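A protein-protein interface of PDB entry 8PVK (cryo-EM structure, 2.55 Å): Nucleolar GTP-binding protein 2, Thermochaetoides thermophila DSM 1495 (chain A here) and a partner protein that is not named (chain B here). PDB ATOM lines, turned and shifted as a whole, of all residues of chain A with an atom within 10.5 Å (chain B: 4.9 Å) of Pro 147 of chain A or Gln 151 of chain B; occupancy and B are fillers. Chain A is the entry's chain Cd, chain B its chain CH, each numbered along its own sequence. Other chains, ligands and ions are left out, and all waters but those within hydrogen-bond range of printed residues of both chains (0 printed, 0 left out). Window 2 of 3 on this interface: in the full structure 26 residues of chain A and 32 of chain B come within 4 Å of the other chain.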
ATOM      1  N   PHE A 141       7.189   0.565 -16.908  1.00  0.00           N
ATOM      2  CA  PHE A 141       5.958  -0.209 -16.773  1.00  0.00           C
ATOM      3  C   PHE A 141       6.000  -1.483 -17.610  1.00  0.00           C
ATOM      4  O   PHE A 141       5.485  -2.526 -17.192  1.00  0.00           O
ATOM      5  CB  PHE A 141       4.757   0.646 -17.177  1.00  0.00           C
ATOM      6  CG  PHE A 141       4.278   1.575 -16.101  1.00  0.00           C
ATOM      7  CD1 PHE A 141       3.659   1.083 -14.964  1.00  0.00           C
ATOM      8  CD2 PHE A 141       4.432   2.945 -16.233  1.00  0.00           C
ATOM      9  CE1 PHE A 141       3.212   1.938 -13.976  1.00  0.00           C
ATOM     10  CE2 PHE A 141       3.987   3.805 -15.249  1.00  0.00           C
ATOM     11  CZ  PHE A 141       3.375   3.301 -14.121  1.00  0.00           C
ATOM     12  N   SER A 142       6.610  -1.417 -18.796  1.00  0.00           N
ATOM     13  CA  SER A 142       6.626  -2.563 -19.698  1.00  0.00           C
ATOM     14  C   SER A 142       7.524  -3.690 -19.205  1.00  0.00           C
ATOM     15  O   SER A 142       7.290  -4.848 -19.562  1.00  0.00           O
ATOM     16  CB  SER A 142       7.065  -2.123 -21.095  1.00  0.00           C
ATOM     17  OG  SER A 142       8.322  -1.471 -21.049  1.00  0.00           O
ATOM     18  N   GLU A 143       8.542  -3.383 -18.403  1.00  0.00           N
ATOM     19  CA  GLU A 143       9.413  -4.409 -17.846  1.00  0.00           C
ATOM     20  C   GLU A 143       8.888  -4.994 -16.545  1.00  0.00           C
ATOM     21  O   GLU A 143       9.471  -5.957 -16.036  1.00  0.00           O
ATOM     22  CB  GLU A 143      10.819  -3.844 -17.615  1.00  0.00           C
ATOM     23  CG  GLU A 143      11.476  -3.284 -18.861  1.00  0.00           C
ATOM     24  CD  GLU A 143      12.881  -2.779 -18.598  1.00  0.00           C
ATOM     25  OE1 GLU A 143      13.361  -2.926 -17.454  1.00  0.00           O
ATOM     26  OE2 GLU A 143      13.502  -2.233 -19.532  1.00  0.00           O
ATOM     27  N   THR A 144       7.810  -4.441 -15.995  1.00  0.00           N
ATOM     28  CA  THR A 144       7.243  -4.903 -14.735  1.00  0.00           C
ATOM     29  C   THR A 144       6.124  -5.916 -14.935  1.00  0.00           C
ATOM     30  O   THR A 144       6.186  -7.025 -14.396  1.00  0.00           O
ATOM     31  CB  THR A 144       6.726  -3.707 -13.929  1.00  0.00           C
ATOM     32  OG1 THR A 144       7.804  -2.799 -13.676  1.00  0.00           O
ATOM     33  CG2 THR A 144       6.144  -4.172 -12.617  1.00  0.00           C
ATOM     34  N   PHE A 145       5.098  -5.558 -15.701  1.00  0.00           N
ATOM     35  CA  PHE A 145       4.001  -6.462 -16.002  1.00  0.00           C
ATOM     36  C   PHE A 145       3.645  -6.331 -17.473  1.00  0.00           C
ATOM     37  O   PHE A 145       3.779  -5.258 -18.066  1.00  0.00           O
ATOM     38  CB  PHE A 145       2.774  -6.172 -15.126  1.00  0.00           C
ATOM     39  CG  PHE A 145       1.808  -7.318 -15.040  1.00  0.00           C
ATOM     40  CD1 PHE A 145       2.077  -8.408 -14.230  1.00  0.00           C
ATOM     41  CD2 PHE A 145       0.631  -7.305 -15.769  1.00  0.00           C
ATOM     42  CE1 PHE A 145       1.190  -9.465 -14.150  1.00  0.00           C
ATOM     43  CE2 PHE A 145      -0.260  -8.356 -15.693  1.00  0.00           C
ATOM     44  CZ  PHE A 145       0.020  -9.437 -14.883  1.00  0.00           C
ATOM     45  N   GLY A 146       3.192  -7.435 -18.060  1.00  0.00           N
ATOM     46  CA  GLY A 146       2.829  -7.455 -19.455  1.00  0.00           C
ATOM     47  C   GLY A 146       3.496  -8.584 -20.211  1.00  0.00           C
ATOM     48  O   GLY A 146       4.193  -9.424 -19.633  1.00  0.00           O
ATOM     49  N   PRO A 147       3.275  -8.634 -21.529  1.00  0.00           N
ATOM     50  CA  PRO A 147       3.875  -9.710 -22.338  1.00  0.00           C
ATOM     51  C   PRO A 147       5.391  -9.653 -22.425  1.00  0.00           C
ATOM     52  O   PRO A 147       6.016 -10.699 -22.637  1.00  0.00           O
ATOM     53  CB  PRO A 147       3.234  -9.512 -23.719  1.00  0.00           C
ATOM     54  CG  PRO A 147       2.774  -8.093 -23.731  1.00  0.00           C
ATOM     55  CD  PRO A 147       2.383  -7.774 -22.324  1.00  0.00           C
ATOM     56  N   LYS A 148       6.002  -8.479 -22.267  1.00  0.00           N
ATOM     57  CA  LYS A 148       7.448  -8.328 -22.376  1.00  0.00           C
ATOM     58  C   LYS A 148       8.097  -7.986 -21.040  1.00  0.00           C
ATOM     59  O   LYS A 148       9.181  -7.395 -21.015  1.00  0.00           O
ATOM     60  CB  LYS A 148       7.795  -7.266 -23.421  1.00  0.00           C
ATOM     61  CG  LYS A 148       7.121  -7.464 -24.771  1.00  0.00           C
ATOM     62  CD  LYS A 148       7.349  -8.867 -25.314  1.00  0.00           C
ATOM     63  CE  LYS A 148       6.345  -9.209 -26.401  1.00  0.00           C
ATOM     64  NZ  LYS A 148       6.318 -10.668 -26.693  1.00  0.00           N
ATOM     65  N   ALA A 149       7.450  -8.338 -19.932  1.00  0.00           N
ATOM     66  CA  ALA A 149       7.988  -8.030 -18.616  1.00  0.00           C
ATOM     67  C   ALA A 149       9.198  -8.901 -18.306  1.00  0.00           C
ATOM     68  O   ALA A 149       9.251 -10.077 -18.675  1.00  0.00           O
ATOM     69  CB  ALA A 149       6.917  -8.227 -17.547  1.00  0.00           C
ATOM     70  N   GLN A 150      10.177  -8.312 -17.620  1.00  0.00           N
ATOM     71  CA  GLN A 150      11.382  -9.020 -17.211  1.00  0.00           C
ATOM     72  C   GLN A 150      11.538  -9.072 -15.697  1.00  0.00           C
ATOM     73  O   GLN A 150      12.609  -9.442 -15.207  1.00  0.00           O
ATOM     74  CB  GLN A 150      12.618  -8.372 -17.842  1.00  0.00           C
ATOM     75  CG  GLN A 150      12.605  -8.360 -19.360  1.00  0.00           C
ATOM     76  CD  GLN A 150      12.582  -9.753 -19.955  1.00  0.00           C
ATOM     77  OE1 GLN A 150      13.400 -10.604 -19.605  1.00  0.00           O
ATOM     78  NE2 GLN A 150      11.644  -9.995 -20.861  1.00  0.00           N
ATOM     79  N   ARG A 151      10.499  -8.713 -14.947  1.00  0.00           N
ATOM     80  CA  ARG A 151      10.573  -8.684 -13.493  1.00  0.00           C
ATOM     81  C   ARG A 151      10.464 -10.102 -12.946  1.00  0.00           C
ATOM     82  O   ARG A 151       9.469 -10.793 -13.185  1.00  0.00           O
ATOM     83  CB  ARG A 151       9.469  -7.792 -12.931  1.00  0.00           C
ATOM     84  CG  ARG A 151       9.197  -7.969 -11.448  1.00  0.00           C
ATOM     85  CD  ARG A 151       8.136  -6.989 -10.981  1.00  0.00           C
ATOM     86  NE  ARG A 151       7.680  -7.267  -9.623  1.00  0.00           N
ATOM     87  CZ  ARG A 151       6.580  -7.943  -9.328  1.00  0.00           C
ATOM     88  NH1 ARG A 151       5.801  -8.443 -10.273  1.00  0.00           N
ATOM     89  NH2 ARG A 151       6.253  -8.125  -8.052  1.00  0.00           N
ATOM     90  N   ILE B 147      -1.496   1.036 -20.549  1.00  0.00           N
ATOM     91  CA  ILE B 147      -1.187  -0.323 -20.992  1.00  0.00           C
ATOM     92  C   ILE B 147      -0.963  -1.235 -19.791  1.00  0.00           C
ATOM     93  O   ILE B 147      -1.483  -2.362 -19.730  1.00  0.00           O
ATOM     94  CB  ILE B 147       0.040  -0.309 -21.923  1.00  0.00           C
ATOM     95  CG1 ILE B 147      -0.234   0.555 -23.154  1.00  0.00           C
ATOM     96  CG2 ILE B 147       0.423  -1.720 -22.335  1.00  0.00           C
ATOM     97  CD1 ILE B 147       1.012   0.929 -23.922  1.00  0.00           C
ATOM     98  N   TYR B 148      -0.195  -0.745 -18.810  1.00  0.00           N
ATOM     99  CA  TYR B 148       0.062  -1.517 -17.598  1.00  0.00           C
ATOM    100  C   TYR B 148      -1.229  -1.822 -16.844  1.00  0.00           C
ATOM    101  O   TYR B 148      -1.434  -2.950 -16.380  1.00  0.00           O
ATOM    102  CB  TYR B 148       1.051  -0.756 -16.711  1.00  0.00           C
ATOM    103  CG  TYR B 148       1.204  -1.298 -15.308  1.00  0.00           C
ATOM    104  CD1 TYR B 148       2.089  -2.332 -15.033  1.00  0.00           C
ATOM    105  CD2 TYR B 148       0.492  -0.746 -14.250  1.00  0.00           C
ATOM    106  CE1 TYR B 148       2.235  -2.818 -13.750  1.00  0.00           C
ATOM    107  CE2 TYR B 148       0.628  -1.227 -12.973  1.00  0.00           C
ATOM    108  CZ  TYR B 148       1.501  -2.258 -12.726  1.00  0.00           C
ATOM    109  OH  TYR B 148       1.633  -2.727 -11.445  1.00  0.00           O
ATOM    110  N   LEU B 149      -2.120  -0.833 -16.734  1.00  0.00           N
ATOM    111  CA  LEU B 149      -3.367  -1.031 -16.010  1.00  0.00           C
ATOM    112  C   LEU B 149      -4.310  -1.964 -16.752  1.00  0.00           C
ATOM    113  O   LEU B 149      -5.053  -2.710 -16.113  1.00  0.00           O
ATOM    114  CB  LEU B 149      -4.042   0.315 -15.746  1.00  0.00           C
ATOM    115  CG  LEU B 149      -3.480   1.113 -14.567  1.00  0.00           C
ATOM    116  CD1 LEU B 149      -4.126   2.486 -14.487  1.00  0.00           C
ATOM    117  CD2 LEU B 149      -3.641   0.357 -13.260  1.00  0.00           C
ATOM    118  N   ASP B 150      -4.287  -1.957 -18.089  1.00  0.00           N
ATOM    119  CA  ASP B 150      -5.098  -2.916 -18.837  1.00  0.00           C
ATOM    120  C   ASP B 150      -4.610  -4.347 -18.630  1.00  0.00           C
ATOM    121  O   ASP B 150      -5.425  -5.268 -18.455  1.00  0.00           O
ATOM    122  CB  ASP B 150      -5.100  -2.559 -20.321  1.00  0.00           C
ATOM    123  CG  ASP B 150      -6.204  -3.264 -21.082  1.00  0.00           C
ATOM    124  OD1 ASP B 150      -7.335  -3.340 -20.556  1.00  0.00           O
ATOM    125  OD2 ASP B 150      -5.943  -3.744 -22.203  1.00  0.00           O
ATOM    126  N   GLN B 151      -3.286  -4.556 -18.641  1.00  0.00           N
ATOM    127  CA  GLN B 151      -2.757  -5.894 -18.368  1.00  0.00           C
ATOM    128  C   GLN B 151      -3.089  -6.349 -16.948  1.00  0.00           C
ATOM    129  O   GLN B 151      -3.484  -7.507 -16.728  1.00  0.00           O
ATOM    130  CB  GLN B 151      -1.245  -5.925 -18.595  1.00  0.00           C
ATOM    131  CG  GLN B 151      -0.808  -5.527 -19.991  1.00  0.00           C
ATOM    132  CD  GLN B 151      -1.255  -6.513 -21.049  1.00  0.00           C
ATOM    133  OE1 GLN B 151      -1.315  -7.718 -20.806  1.00  0.00           O
ATOM    134  NE2 GLN B 151      -1.574  -6.005 -22.232  1.00  0.00           N
ATOM    135  N   VAL B 152      -2.948  -5.439 -15.978  1.00  0.00           N
ATOM    136  CA  VAL B 152      -3.278  -5.744 -14.588  1.00  0.00           C
ATOM    137  C   VAL B 152      -4.765  -6.058 -14.446  1.00  0.00           C
ATOM    138  O   VAL B 152      -5.153  -6.966 -13.702  1.00  0.00           O
ATOM    139  CB  VAL B 152      -2.832  -4.579 -13.680  1.00  0.00           C
ATOM    140  CG1 VAL B 152      -3.473  -4.655 -12.304  1.00  0.00           C
ATOM    141  CG2 VAL B 152      -1.319  -4.571 -13.545  1.00  0.00           C
ATOM    142  N   ARG B 153      -5.614  -5.339 -15.189  1.00  0.00           N
ATOM    143  CA  ARG B 153      -7.053  -5.584 -15.154  1.00  0.00           C
ATOM    144  C   ARG B 153      -7.403  -6.966 -15.693  1.00  0.00           C
ATOM    145  O   ARG B 153      -8.242  -7.666 -15.116  1.00  0.00           O
ATOM    146  CB  ARG B 153      -7.781  -4.505 -15.956  1.00  0.00           C
ATOM    147  CG  ARG B 153      -9.253  -4.791 -16.191  1.00  0.00           C
ATOM    148  CD  ARG B 153      -9.782  -4.022 -17.381  1.00  0.00           C
ATOM    149  NE  ARG B 153      -9.403  -4.620 -18.655  1.00  0.00           N
ATOM    150  CZ  ARG B 153     -10.113  -5.542 -19.290  1.00  0.00           C
ATOM    151  NH1 ARG B 153     -11.240  -6.016 -18.786  1.00  0.00           N
ATOM    152  NH2 ARG B 153      -9.680  -6.000 -20.461  1.00  0.00           N
ATOM    153  N   GLN B 154      -6.774  -7.373 -16.799  1.00  0.00           N
ATOM    154  CA  GLN B 154      -7.047  -8.703 -17.343  1.00  0.00           C
ATOM    155  C   GLN B 154      -6.599  -9.807 -16.385  1.00  0.00           C
ATOM    156  O   GLN B 154      -7.334 -10.782 -16.161  1.00  0.00           O
ATOM    157  CB  GLN B 154      -6.378  -8.865 -18.705  1.00  0.00           C
ATOM    158  CG  GLN B 154      -7.009  -8.022 -19.793  1.00  0.00           C
ATOM    159  CD  GLN B 154      -6.549  -8.418 -21.177  1.00  0.00           C
ATOM    160  OE1 GLN B 154      -5.845  -9.411 -21.350  1.00  0.00           O
ATOM    161  NE2 GLN B 154      -6.949  -7.642 -22.177  1.00  0.00           N
ATOM    162  N   HIS B 155      -5.412  -9.654 -15.788  1.00  0.00           N
ATOM    163  CA  HIS B 155      -4.944 -10.656 -14.832  1.00  0.00           C
ATOM    164  C   HIS B 155      -5.834 -10.701 -13.590  1.00  0.00           C
ATOM    165  O   HIS B 155      -6.118 -11.783 -13.059  1.00  0.00           O
ATOM    166  CB  HIS B 155      -3.491 -10.383 -14.448  1.00  0.00           C
ATOM    167  CG  HIS B 155      -2.805 -11.554 -13.815  1.00  0.00           C
ATOM    168  ND1 HIS B 155      -2.747 -11.736 -12.451  1.00  0.00           N
ATOM    169  CD2 HIS B 155      -2.151 -12.606 -14.363  1.00  0.00           C
ATOM    170  CE1 HIS B 155      -2.084 -12.847 -12.185  1.00  0.00           C
ATOM    171  NE2 HIS B 155      -1.713 -13.394 -13.327  1.00  0.00           N
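Among the printed residues, pairs that only touch across the chains: Phe 141 of chain A with Tyr 148 of chain B (3.4 Å), Phe 145 of chain A with Tyr 148 of chain B (3.7 Å), Phe 145 of chain A with Gln 151 of chain B (3.5 Å), Phe 145 of chain A with Val 152 of chain B (3.98 Å), Phe 145 of chain A with His 155 of chain B (3.7 Å) and Pro 147 of chain A with Gln 151 of chain B (3.998 Å).
Of the printed residues of chain B, Pro 147 of chain A touches Gln 151 (3.998 Å). Of the printed residues of chain A, Gln 151 of chain B touches Phe 145 (3.5 Å) and Pro 147 (3.998 Å). Of chain A, only Phe 145 comes within 4 Å of Val 152 of chain B. No residue of chain A comes within 4 Å of Gln 154 of chain B. Of the printed residues of chain B, Phe 141 of chain A touches Tyr 148 (3.4 Å). Of the printed residues of chain B, Phe 145 of chain A touches Tyr 148, Gln 151, Val 152 and His 155. Printed residues of chain A within 4 Å of His 155 of chain B: Phe 145. Of the printed residues of chain A, Tyr 148 of chain B touches Phe 141 (3.4 Å) and Phe 145 (3.7 Å). The nearest printed residue of chain B that does not touch Pro 147 of chain A is Ile 147 of chain B (6.4 Å). The nearest printed residue of chain A that does not touch Gln 151 of chain B is Gly 146 of chain A (4.2 Å). The nearest printed residue of chain B that does not touch Phe 141 of chain A is Leu 149 of chain B (6.3 Å).
Hydrophobic or aromatic side chains of chain B within 4 Å of the printed part of chain A: Tyr 148 and His 155. Among the printed residues, no Asp or Glu carboxylate lies within 4 Å of a Lys or Arg side-chain nitrogen of the other chain.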
